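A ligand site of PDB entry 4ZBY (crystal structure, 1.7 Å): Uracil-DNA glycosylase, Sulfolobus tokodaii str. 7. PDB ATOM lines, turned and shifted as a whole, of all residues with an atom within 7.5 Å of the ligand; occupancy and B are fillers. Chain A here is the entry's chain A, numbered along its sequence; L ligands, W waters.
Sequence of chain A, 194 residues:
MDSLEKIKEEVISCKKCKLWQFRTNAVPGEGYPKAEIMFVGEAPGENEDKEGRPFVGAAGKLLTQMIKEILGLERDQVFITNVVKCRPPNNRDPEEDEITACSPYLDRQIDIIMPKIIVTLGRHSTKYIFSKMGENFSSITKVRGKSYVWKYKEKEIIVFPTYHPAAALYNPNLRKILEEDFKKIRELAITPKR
The side-chain amide oxygen (OD1) of Asn 82 lies within hydrogen-bond range of a nitrogen (N2) of the ligand (2.7 Å). NE2 of His 164 sits at hydrogen-bond distance from O1 of the ligand, 2.8 Å away. O1 of the ligand is in hydrogen-bond range of N of Glu 42 (2.9 Å). N of Phe 55 lies within hydrogen-bond range of O2 of the ligand, at 2.9 Å. The backbone NH (N) of Ala 43 is in hydrogen-bond range of an oxygen (O1) of the ligand (3.3 Å). A nitrogen (N2) of the ligand lies close to the backbone carbonyl oxygen (O) of Ala 43.
The side-chain amide oxygen (OD1) of Asn 82 is in hydrogen-bond range of the backbone NH (N) of Glu 42 (3.3 Å). N of Gly 41 sits close to OD1 of Asn 82, 3.4 Å away. The backbone NH of Ala 166 sits at hydrogen-bond distance from a ring nitrogen (ND1) of His 164, at 3.0 Å. O of Glu 48 lies within hydrogen-bond range of N of Arg 53. The side-chain carboxylate of Glu 48 is in hydrogen-bond range of the backbone NH of Val 56, 2.8 Å away. OE2 of Glu 48 lies within hydrogen-bond range of N of Gly 57, 3.0 Å away. O of Thr 81 lies within hydrogen-bond range of N of Gly 41 (2.8 Å). The backbone NH of Val 83 sits at hydrogen-bond distance from the backbone carbonyl oxygen of Gly 41, 3.0 Å away.
Merely in contact with the ligand: Glu 48, Pro 54, Gly 41 and Gly 45. Hydrophobic or aromatic side chains within 4 Å of the ligand: Pro 54, Phe 55 and His 164. The nearest printed residue that does not touch the ligand is Pro 44 (4.1 Å).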
ATOM      1  N   VAL A  27     -28.398  16.230  15.225  1.00  0.00           N
ATOM      2  CA  VAL A  27     -28.629  16.610  13.831  1.00  0.00           C
ATOM      3  C   VAL A  27     -27.887  15.654  12.906  1.00  0.00           C
ATOM      4  O   VAL A  27     -26.698  15.895  12.581  1.00  0.00           O
ATOM      5  CB  VAL A  27     -28.137  18.072  13.580  1.00  0.00           C
ATOM      6  CG1 VAL A  27     -28.449  18.524  12.166  1.00  0.00           C
ATOM      7  CG2 VAL A  27     -28.796  19.059  14.593  1.00  0.00           C
ATOM      8  N   VAL A  40     -20.567  19.005   3.845  1.00  0.00           N
ATOM      9  CA  VAL A  40     -20.231  18.675   5.238  1.00  0.00           C
ATOM     10  C   VAL A  40     -19.716  19.883   5.961  1.00  0.00           C
ATOM     11  O   VAL A  40     -18.683  20.441   5.595  1.00  0.00           O
ATOM     12  CB  VAL A  40     -19.152  17.560   5.313  1.00  0.00           C
ATOM     13  CG1 VAL A  40     -18.928  17.110   6.754  1.00  0.00           C
ATOM     14  CG2 VAL A  40     -19.543  16.374   4.431  1.00  0.00           C
ATOM     15  N   GLY A  41     -20.447  20.300   6.997  1.00  0.00           N
ATOM     16  CA  GLY A  41     -19.988  21.383   7.845  1.00  0.00           C
ATOM     17  C   GLY A  41     -19.298  20.911   9.112  1.00  0.00           C
ATOM     18  O   GLY A  41     -18.886  19.765   9.246  1.00  0.00           O
ATOM     19  N   GLU A  42     -19.170  21.839  10.054  1.00  0.00           N
ATOM     20  CA  GLU A  42     -18.489  21.596  11.325  1.00  0.00           C
ATOM     21  C   GLU A  42     -19.382  20.905  12.363  1.00  0.00           C
ATOM     22  O   GLU A  42     -19.157  19.740  12.740  1.00  0.00           O
ATOM     23  CB  GLU A  42     -17.971  22.921  11.889  1.00  0.00           C
ATOM     24  CG  GLU A  42     -17.319  22.793  13.269  1.00  0.00           C
ATOM     25  CD  GLU A  42     -16.918  24.126  13.866  1.00  0.00           C
ATOM     26  OE1 GLU A  42     -17.030  25.171  13.166  1.00  0.00           O
ATOM     27  OE2 GLU A  42     -16.480  24.134  15.031  1.00  0.00           O
ATOM     28  N   ALA A  43     -20.377  21.637  12.834  1.00  0.00           N
ATOM     29  CA  ALA A  43     -21.299  21.152  13.863  1.00  0.00           C
ATOM     30  C   ALA A  43     -22.529  22.033  13.858  1.00  0.00           C
ATOM     31  O   ALA A  43     -22.470  23.191  13.388  1.00  0.00           O
ATOM     32  CB  ALA A  43     -20.616  21.130  15.254  1.00  0.00           C
ATOM     33  N   PRO A  44     -23.640  21.526  14.391  1.00  0.00           N
ATOM     34  CA  PRO A  44     -24.860  22.329  14.525  1.00  0.00           C
ATOM     35  C   PRO A  44     -24.643  23.596  15.315  1.00  0.00           C
ATOM     36  O   PRO A  44     -23.914  23.609  16.316  1.00  0.00           O
ATOM     37  CB  PRO A  44     -25.815  21.400  15.303  1.00  0.00           C
ATOM     38  CG  PRO A  44     -25.299  20.052  15.116  1.00  0.00           C
ATOM     39  CD  PRO A  44     -23.832  20.131  14.848  1.00  0.00           C
ATOM     40  N   GLY A  45     -25.306  24.671  14.896  1.00  0.00           N
ATOM     41  CA  GLY A  45     -25.416  25.813  15.770  1.00  0.00           C
ATOM     42  C   GLY A  45     -26.733  25.823  16.526  1.00  0.00           C
ATOM     43  O   GLY A  45     -27.401  24.801  16.669  1.00  0.00           O
ATOM     44  N   GLU A  46     -27.104  27.001  17.011  1.00  0.00           N
ATOM     45  CA  GLU A  46     -28.279  27.140  17.861  1.00  0.00           C
ATOM     46  C   GLU A  46     -29.582  26.739  17.166  1.00  0.00           C
ATOM     47  O   GLU A  46     -30.406  26.014  17.733  1.00  0.00           O
ATOM     48  CB  GLU A  46     -28.389  28.600  18.359  1.00  0.00           C
ATOM     49  CG  GLU A  46     -29.538  28.848  19.298  1.00  0.00           C
ATOM     50  CD  GLU A  46     -29.594  30.288  19.795  1.00  0.00           C
ATOM     51  OE1 GLU A  46     -28.779  31.116  19.326  1.00  0.00           O
ATOM     52  OE2 GLU A  46     -30.452  30.591  20.646  1.00  0.00           O
ATOM     53  N   ASN A  47     -29.813  27.243  15.950  1.00  0.00           N
ATOM     54  CA  ASN A  47     -31.068  26.955  15.273  1.00  0.00           C
ATOM     55  C   ASN A  47     -31.127  25.501  14.830  1.00  0.00           C
ATOM     56  O   ASN A  47     -32.189  24.883  14.816  1.00  0.00           O
ATOM     57  CB  ASN A  47     -31.265  27.875  14.071  1.00  0.00           C
ATOM     58  CG  ASN A  47     -31.401  29.324  14.490  1.00  0.00           C
ATOM     59  OD1 ASN A  47     -30.654  30.197  14.031  1.00  0.00           O
ATOM     60  ND2 ASN A  47     -32.339  29.593  15.384  1.00  0.00           N
ATOM     61  N   GLU A  48     -29.975  24.963  14.458  1.00  0.00           N
ATOM     62  CA  GLU A  48     -29.891  23.561  14.066  1.00  0.00           C
ATOM     63  C   GLU A  48     -30.279  22.653  15.233  1.00  0.00           C
ATOM     64  O   GLU A  48     -31.006  21.690  15.066  1.00  0.00           O
ATOM     65  CB  GLU A  48     -28.471  23.223  13.588  1.00  0.00           C
ATOM     66  CG  GLU A  48     -28.125  23.844  12.236  1.00  0.00           C
ATOM     67  CD  GLU A  48     -27.890  25.340  12.304  1.00  0.00           C
ATOM     68  OE1 GLU A  48     -27.509  25.882  13.396  1.00  0.00           O
ATOM     69  OE2 GLU A  48     -28.097  25.996  11.266  1.00  0.00           O
ATOM     70  N   ASP A  49     -29.758  22.963  16.409  1.00  0.00           N
ATOM     71  CA  ASP A  49     -30.076  22.241  17.636  1.00  0.00           C
ATOM     72  C   ASP A  49     -31.565  22.290  17.941  1.00  0.00           C
ATOM     73  O   ASP A  49     -32.181  21.287  18.278  1.00  0.00           O
ATOM     74  CB  ASP A  49     -29.241  22.850  18.786  1.00  0.00           C
ATOM     75  CG  ASP A  49     -29.545  22.232  20.145  1.00  0.00           C
ATOM     76  OD1 ASP A  49     -29.447  21.012  20.293  1.00  0.00           O
ATOM     77  OD2 ASP A  49     -29.866  22.994  21.080  1.00  0.00           O
ATOM     78  N   ARG A  53     -32.067  19.930  12.398  1.00  0.00           N
ATOM     79  CA  ARG A  53     -31.806  20.024  10.953  1.00  0.00           C
ATOM     80  C   ARG A  53     -30.511  20.783  10.736  1.00  0.00           C
ATOM     81  O   ARG A  53     -30.240  21.702  11.469  1.00  0.00           O
ATOM     82  CB  ARG A  53     -32.945  20.762  10.247  1.00  0.00           C
ATOM     83  CG  ARG A  53     -34.345  20.315  10.615  1.00  0.00           C
ATOM     84  CD  ARG A  53     -35.321  21.083   9.790  1.00  0.00           C
ATOM     85  NE  ARG A  53     -34.877  21.055   8.398  1.00  0.00           N
ATOM     86  CZ  ARG A  53     -35.261  21.928   7.474  1.00  0.00           C
ATOM     87  NH1 ARG A  53     -36.132  22.897   7.779  1.00  0.00           N
ATOM     88  NH2 ARG A  53     -34.788  21.822   6.232  1.00  0.00           N
ATOM     89  N   PRO A  54     -29.714  20.412   9.715  1.00  0.00           N
ATOM     90  CA  PRO A  54     -28.456  21.116   9.476  1.00  0.00           C
ATOM     91  C   PRO A  54     -28.666  22.420   8.702  1.00  0.00           C
ATOM     92  O   PRO A  54     -29.611  22.535   7.911  1.00  0.00           O
ATOM     93  CB  PRO A  54     -27.638  20.116   8.652  1.00  0.00           C
ATOM     94  CG  PRO A  54     -28.680  19.378   7.882  1.00  0.00           C
ATOM     95  CD  PRO A  54     -29.906  19.277   8.783  1.00  0.00           C
ATOM     96  N   PHE A  55     -27.785  23.390   8.942  1.00  0.00           N
ATOM     97  CA  PHE A  55     -27.737  24.614   8.148  1.00  0.00           C
ATOM     98  C   PHE A  55     -29.124  25.256   7.932  1.00  0.00           C
ATOM     99  O   PHE A  55     -29.640  25.381   6.797  1.00  0.00           O
ATOM    100  CB  PHE A  55     -27.032  24.304   6.813  1.00  0.00           C
ATOM    101  CG  PHE A  55     -25.514  24.193   6.945  1.00  0.00           C
ATOM    102  CD1 PHE A  55     -24.751  25.323   7.197  1.00  0.00           C
ATOM    103  CD2 PHE A  55     -24.875  22.968   6.845  1.00  0.00           C
ATOM    104  CE1 PHE A  55     -23.376  25.244   7.306  1.00  0.00           C
ATOM    105  CE2 PHE A  55     -23.502  22.883   6.966  1.00  0.00           C
ATOM    106  CZ  PHE A  55     -22.750  24.007   7.191  1.00  0.00           C
ATOM    107  N   VAL A  56     -29.720  25.707   9.033  1.00  0.00           N
ATOM    108  CA  VAL A  56     -31.027  26.389   8.970  1.00  0.00           C
ATOM    109  C   VAL A  56     -31.002  27.806   9.562  1.00  0.00           C
ATOM    110  O   VAL A  56     -31.981  28.545   9.464  1.00  0.00           O
ATOM    111  CB  VAL A  56     -32.143  25.576   9.672  1.00  0.00           C
ATOM    112  CG1 VAL A  56     -32.533  24.386   8.827  1.00  0.00           C
ATOM    113  CG2 VAL A  56     -31.758  25.135  11.094  1.00  0.00           C
ATOM    114  N   GLY A  57     -29.911  28.159  10.205  1.00  0.00           N
ATOM    115  CA  GLY A  57     -29.741  29.515  10.715  1.00  0.00           C
ATOM    116  C   GLY A  57     -29.265  30.422   9.592  1.00  0.00           C
ATOM    117  O   GLY A  57     -29.358  30.065   8.421  1.00  0.00           O
ATOM    118  N   ALA A  59     -26.248  31.323   8.503  1.00  0.00           N
ATOM    119  CA  ALA A  59     -25.241  30.733   7.644  1.00  0.00           C
ATOM    120  C   ALA A  59     -25.881  29.684   6.753  1.00  0.00           C
ATOM    121  O   ALA A  59     -25.551  29.571   5.571  1.00  0.00           O
ATOM    122  CB  ALA A  59     -24.128  30.115   8.445  1.00  0.00           C
ATOM    123  N   GLY A  60     -26.786  28.905   7.323  1.00  0.00           N
ATOM    124  CA  GLY A  60     -27.477  27.918   6.537  1.00  0.00           C
ATOM    125  C   GLY A  60     -28.353  28.473   5.417  1.00  0.00           C
ATOM    126  O   GLY A  60     -28.448  27.864   4.339  1.00  0.00           O
ATOM    127  N   LEU A  63     -26.124  29.276   2.660  1.00  0.00           N
ATOM    128  CA  LEU A  63     -25.774  28.038   1.975  1.00  0.00           C
ATOM    129  C   LEU A  63     -26.905  27.616   1.033  1.00  0.00           C
ATOM    130  O   LEU A  63     -26.651  27.320  -0.130  1.00  0.00           O
ATOM    131  CB  LEU A  63     -25.486  26.911   2.969  1.00  0.00           C
ATOM    132  CG  LEU A  63     -25.220  25.560   2.308  1.00  0.00           C
ATOM    133  CD1 LEU A  63     -23.954  25.581   1.456  1.00  0.00           C
ATOM    134  CD2 LEU A  63     -25.093  24.457   3.343  1.00  0.00           C
ATOM    135  N   ILE A  80     -26.801  16.990   3.149  1.00  0.00           N
ATOM    136  CA  ILE A  80     -26.124  18.005   3.976  1.00  0.00           C
ATOM    137  C   ILE A  80     -25.968  17.491   5.395  1.00  0.00           C
ATOM    138  O   ILE A  80     -26.949  17.045   6.004  1.00  0.00           O
ATOM    139  CB  ILE A  80     -26.930  19.320   4.020  1.00  0.00           C
ATOM    140  CG1 ILE A  80     -27.077  19.911   2.613  1.00  0.00           C
ATOM    141  CG2 ILE A  80     -26.262  20.299   4.986  1.00  0.00           C
ATOM    142  CD1 ILE A  80     -28.071  21.120   2.568  1.00  0.00           C
ATOM    143  N   THR A  81     -24.747  17.506   5.910  1.00  0.00           N
ATOM    144  CA  THR A  81     -24.527  17.073   7.271  1.00  0.00           C
ATOM    145  C   THR A  81     -23.292  17.774   7.821  1.00  0.00           C
ATOM    146  O   THR A  81     -22.829  18.758   7.250  1.00  0.00           O
ATOM    147  CB  THR A  81     -24.427  15.531   7.351  1.00  0.00           C
ATOM    148  OG1 THR A  81     -24.386  15.129   8.730  1.00  0.00           O
ATOM    149  CG2 THR A  81     -23.197  15.008   6.624  1.00  0.00           C
ATOM    150  N   ASN A  82     -22.795  17.291   8.961  1.00  0.00           N
ATOM    151  CA  ASN A  82     -21.643  17.866   9.646  1.00  0.00           C
ATOM    152  C   ASN A  82     -20.758  16.760  10.186  1.00  0.00           C
ATOM    153  O   ASN A  82     -21.213  15.649  10.385  1.00  0.00           O
ATOM    154  CB  ASN A  82     -22.066  18.756  10.823  1.00  0.00           C
ATOM    155  CG  ASN A  82     -22.855  19.976  10.393  1.00  0.00           C
ATOM    156  OD1 ASN A  82     -22.298  20.913   9.840  1.00  0.00           O
ATOM    157  ND2 ASN A  82     -24.151  19.976  10.659  1.00  0.00           N
ATOM    158  N   VAL A  83     -19.502  17.084  10.475  1.00  0.00           N
ATOM    159  CA  VAL A  83     -18.584  16.089  11.014  1.00  0.00           C
ATOM    160  C   VAL A  83     -18.976  15.736  12.467  1.00  0.00           C
ATOM    161  O   VAL A  83     -18.815  14.579  12.892  1.00  0.00           O
ATOM    162  CB  VAL A  83     -17.120  16.566  10.925  1.00  0.00           C
ATOM    163  CG1 VAL A  83     -16.913  17.848  11.728  1.00  0.00           C
ATOM    164  CG2 VAL A  83     -16.153  15.480  11.369  1.00  0.00           C
ATOM    165  N   VAL A  84     -19.512  16.701  13.208  1.00  0.00           N
ATOM    166  CA  VAL A  84     -20.037  16.460  14.542  1.00  0.00           C
ATOM    167  C   VAL A  84     -21.523  16.790  14.509  1.00  0.00           C
ATOM    168  O   VAL A  84     -21.929  17.773  13.886  1.00  0.00           O
ATOM    169  CB  VAL A  84     -19.295  17.306  15.594  1.00  0.00           C
ATOM    170  CG1 VAL A  84     -20.039  17.346  16.915  1.00  0.00           C
ATOM    171  CG2 VAL A  84     -17.891  16.724  15.785  1.00  0.00           C
ATOM    172  N   LEU A 121     -17.158  22.344   3.939  1.00  0.00           N
ATOM    173  CA  LEU A 121     -17.399  23.723   4.320  1.00  0.00           C
ATOM    174  C   LEU A 121     -16.630  24.042   5.592  1.00  0.00           C
ATOM    175  O   LEU A 121     -17.078  23.696   6.697  1.00  0.00           O
ATOM    176  CB  LEU A 121     -18.908  23.972   4.530  1.00  0.00           C
ATOM    177  CG  LEU A 121     -19.849  23.657   3.359  1.00  0.00           C
ATOM    178  CD1 LEU A 121     -21.308  23.609   3.867  1.00  0.00           C
ATOM    179  CD2 LEU A 121     -19.676  24.717   2.265  1.00  0.00           C
ATOM    180  N   SER A 125     -14.251  20.307   8.818  1.00  0.00           N
ATOM    181  CA  SER A 125     -14.688  19.218   7.948  1.00  0.00           C
ATOM    182  C   SER A 125     -13.608  18.939   6.915  1.00  0.00           C
ATOM    183  O   SER A 125     -13.343  17.775   6.560  1.00  0.00           O
ATOM    184  CB  SER A 125     -16.033  19.562   7.274  1.00  0.00           C
ATOM    185  OG  SER A 125     -15.864  20.687   6.448  1.00  0.00           O
ATOM    186  N   HIS A 164     -16.340  28.388   5.314  1.00  0.00           N
ATOM    187  CA  HIS A 164     -17.627  28.087   5.870  1.00  0.00           C
ATOM    188  C   HIS A 164     -18.569  29.249   5.563  1.00  0.00           C
ATOM    189  O   HIS A 164     -18.155  30.397   5.577  1.00  0.00           O
ATOM    190  CB  HIS A 164     -17.479  27.892   7.379  1.00  0.00           C
ATOM    191  CG  HIS A 164     -18.703  27.352   8.020  1.00  0.00           C
ATOM    192  ND1 HIS A 164     -19.805  28.135   8.303  1.00  0.00           N
ATOM    193  CD2 HIS A 164     -18.984  26.109   8.483  1.00  0.00           C
ATOM    194  CE1 HIS A 164     -20.721  27.390   8.902  1.00  0.00           C
ATOM    195  NE2 HIS A 164     -20.253  26.157   9.014  1.00  0.00           N
ATOM    196  N   PRO A 165     -19.852  28.953   5.322  1.00  0.00           N
ATOM    197  CA  PRO A 165     -20.795  30.021   4.967  1.00  0.00           C
ATOM    198  C   PRO A 165     -20.902  31.118   6.024  1.00  0.00           C
ATOM    199  O   PRO A 165     -21.129  32.262   5.676  1.00  0.00           O
ATOM    200  CB  PRO A 165     -22.123  29.289   4.841  1.00  0.00           C
ATOM    201  CG  PRO A 165     -21.755  27.907   4.524  1.00  0.00           C
ATOM    202  CD  PRO A 165     -20.443  27.616   5.161  1.00  0.00           C
ATOM    203  N   ALA A 166     -20.780  30.748   7.289  1.00  0.00           N
ATOM    204  CA  ALA A 166     -20.823  31.727   8.375  1.00  0.00           C
ATOM    205  C   ALA A 166     -19.763  32.803   8.182  1.00  0.00           C
ATOM    206  O   ALA A 166     -19.984  33.962   8.549  1.00  0.00           O
ATOM    207  CB  ALA A 166     -20.641  31.019   9.690  1.00  0.00           C
HETATM  208  N1  LIG L   1     -22.632  25.482  11.003  1.00  0.00           N
HETATM  209  C1  LIG L   1     -22.270  24.252  10.580  1.00  0.00           C
HETATM  210  O1  LIG L   1     -21.103  23.893  10.513  1.00  0.00           O
HETATM  211  N2  LIG L   1     -23.259  23.363  10.421  1.00  0.00           N
HETATM  212  C2  LIG L   1     -24.571  23.574  10.636  1.00  0.00           C
HETATM  213  O2  LIG L   1     -25.372  22.696  10.378  1.00  0.00           O
HETATM  214  C3  LIG L   1     -24.920  24.878  11.062  1.00  0.00           C
HETATM  215  C4  LIG L   1     -23.953  25.811  11.229  1.00  0.00           C
HETATM  216  O   HOH W   1     -20.518  26.664  12.491  1.00  0.00           O
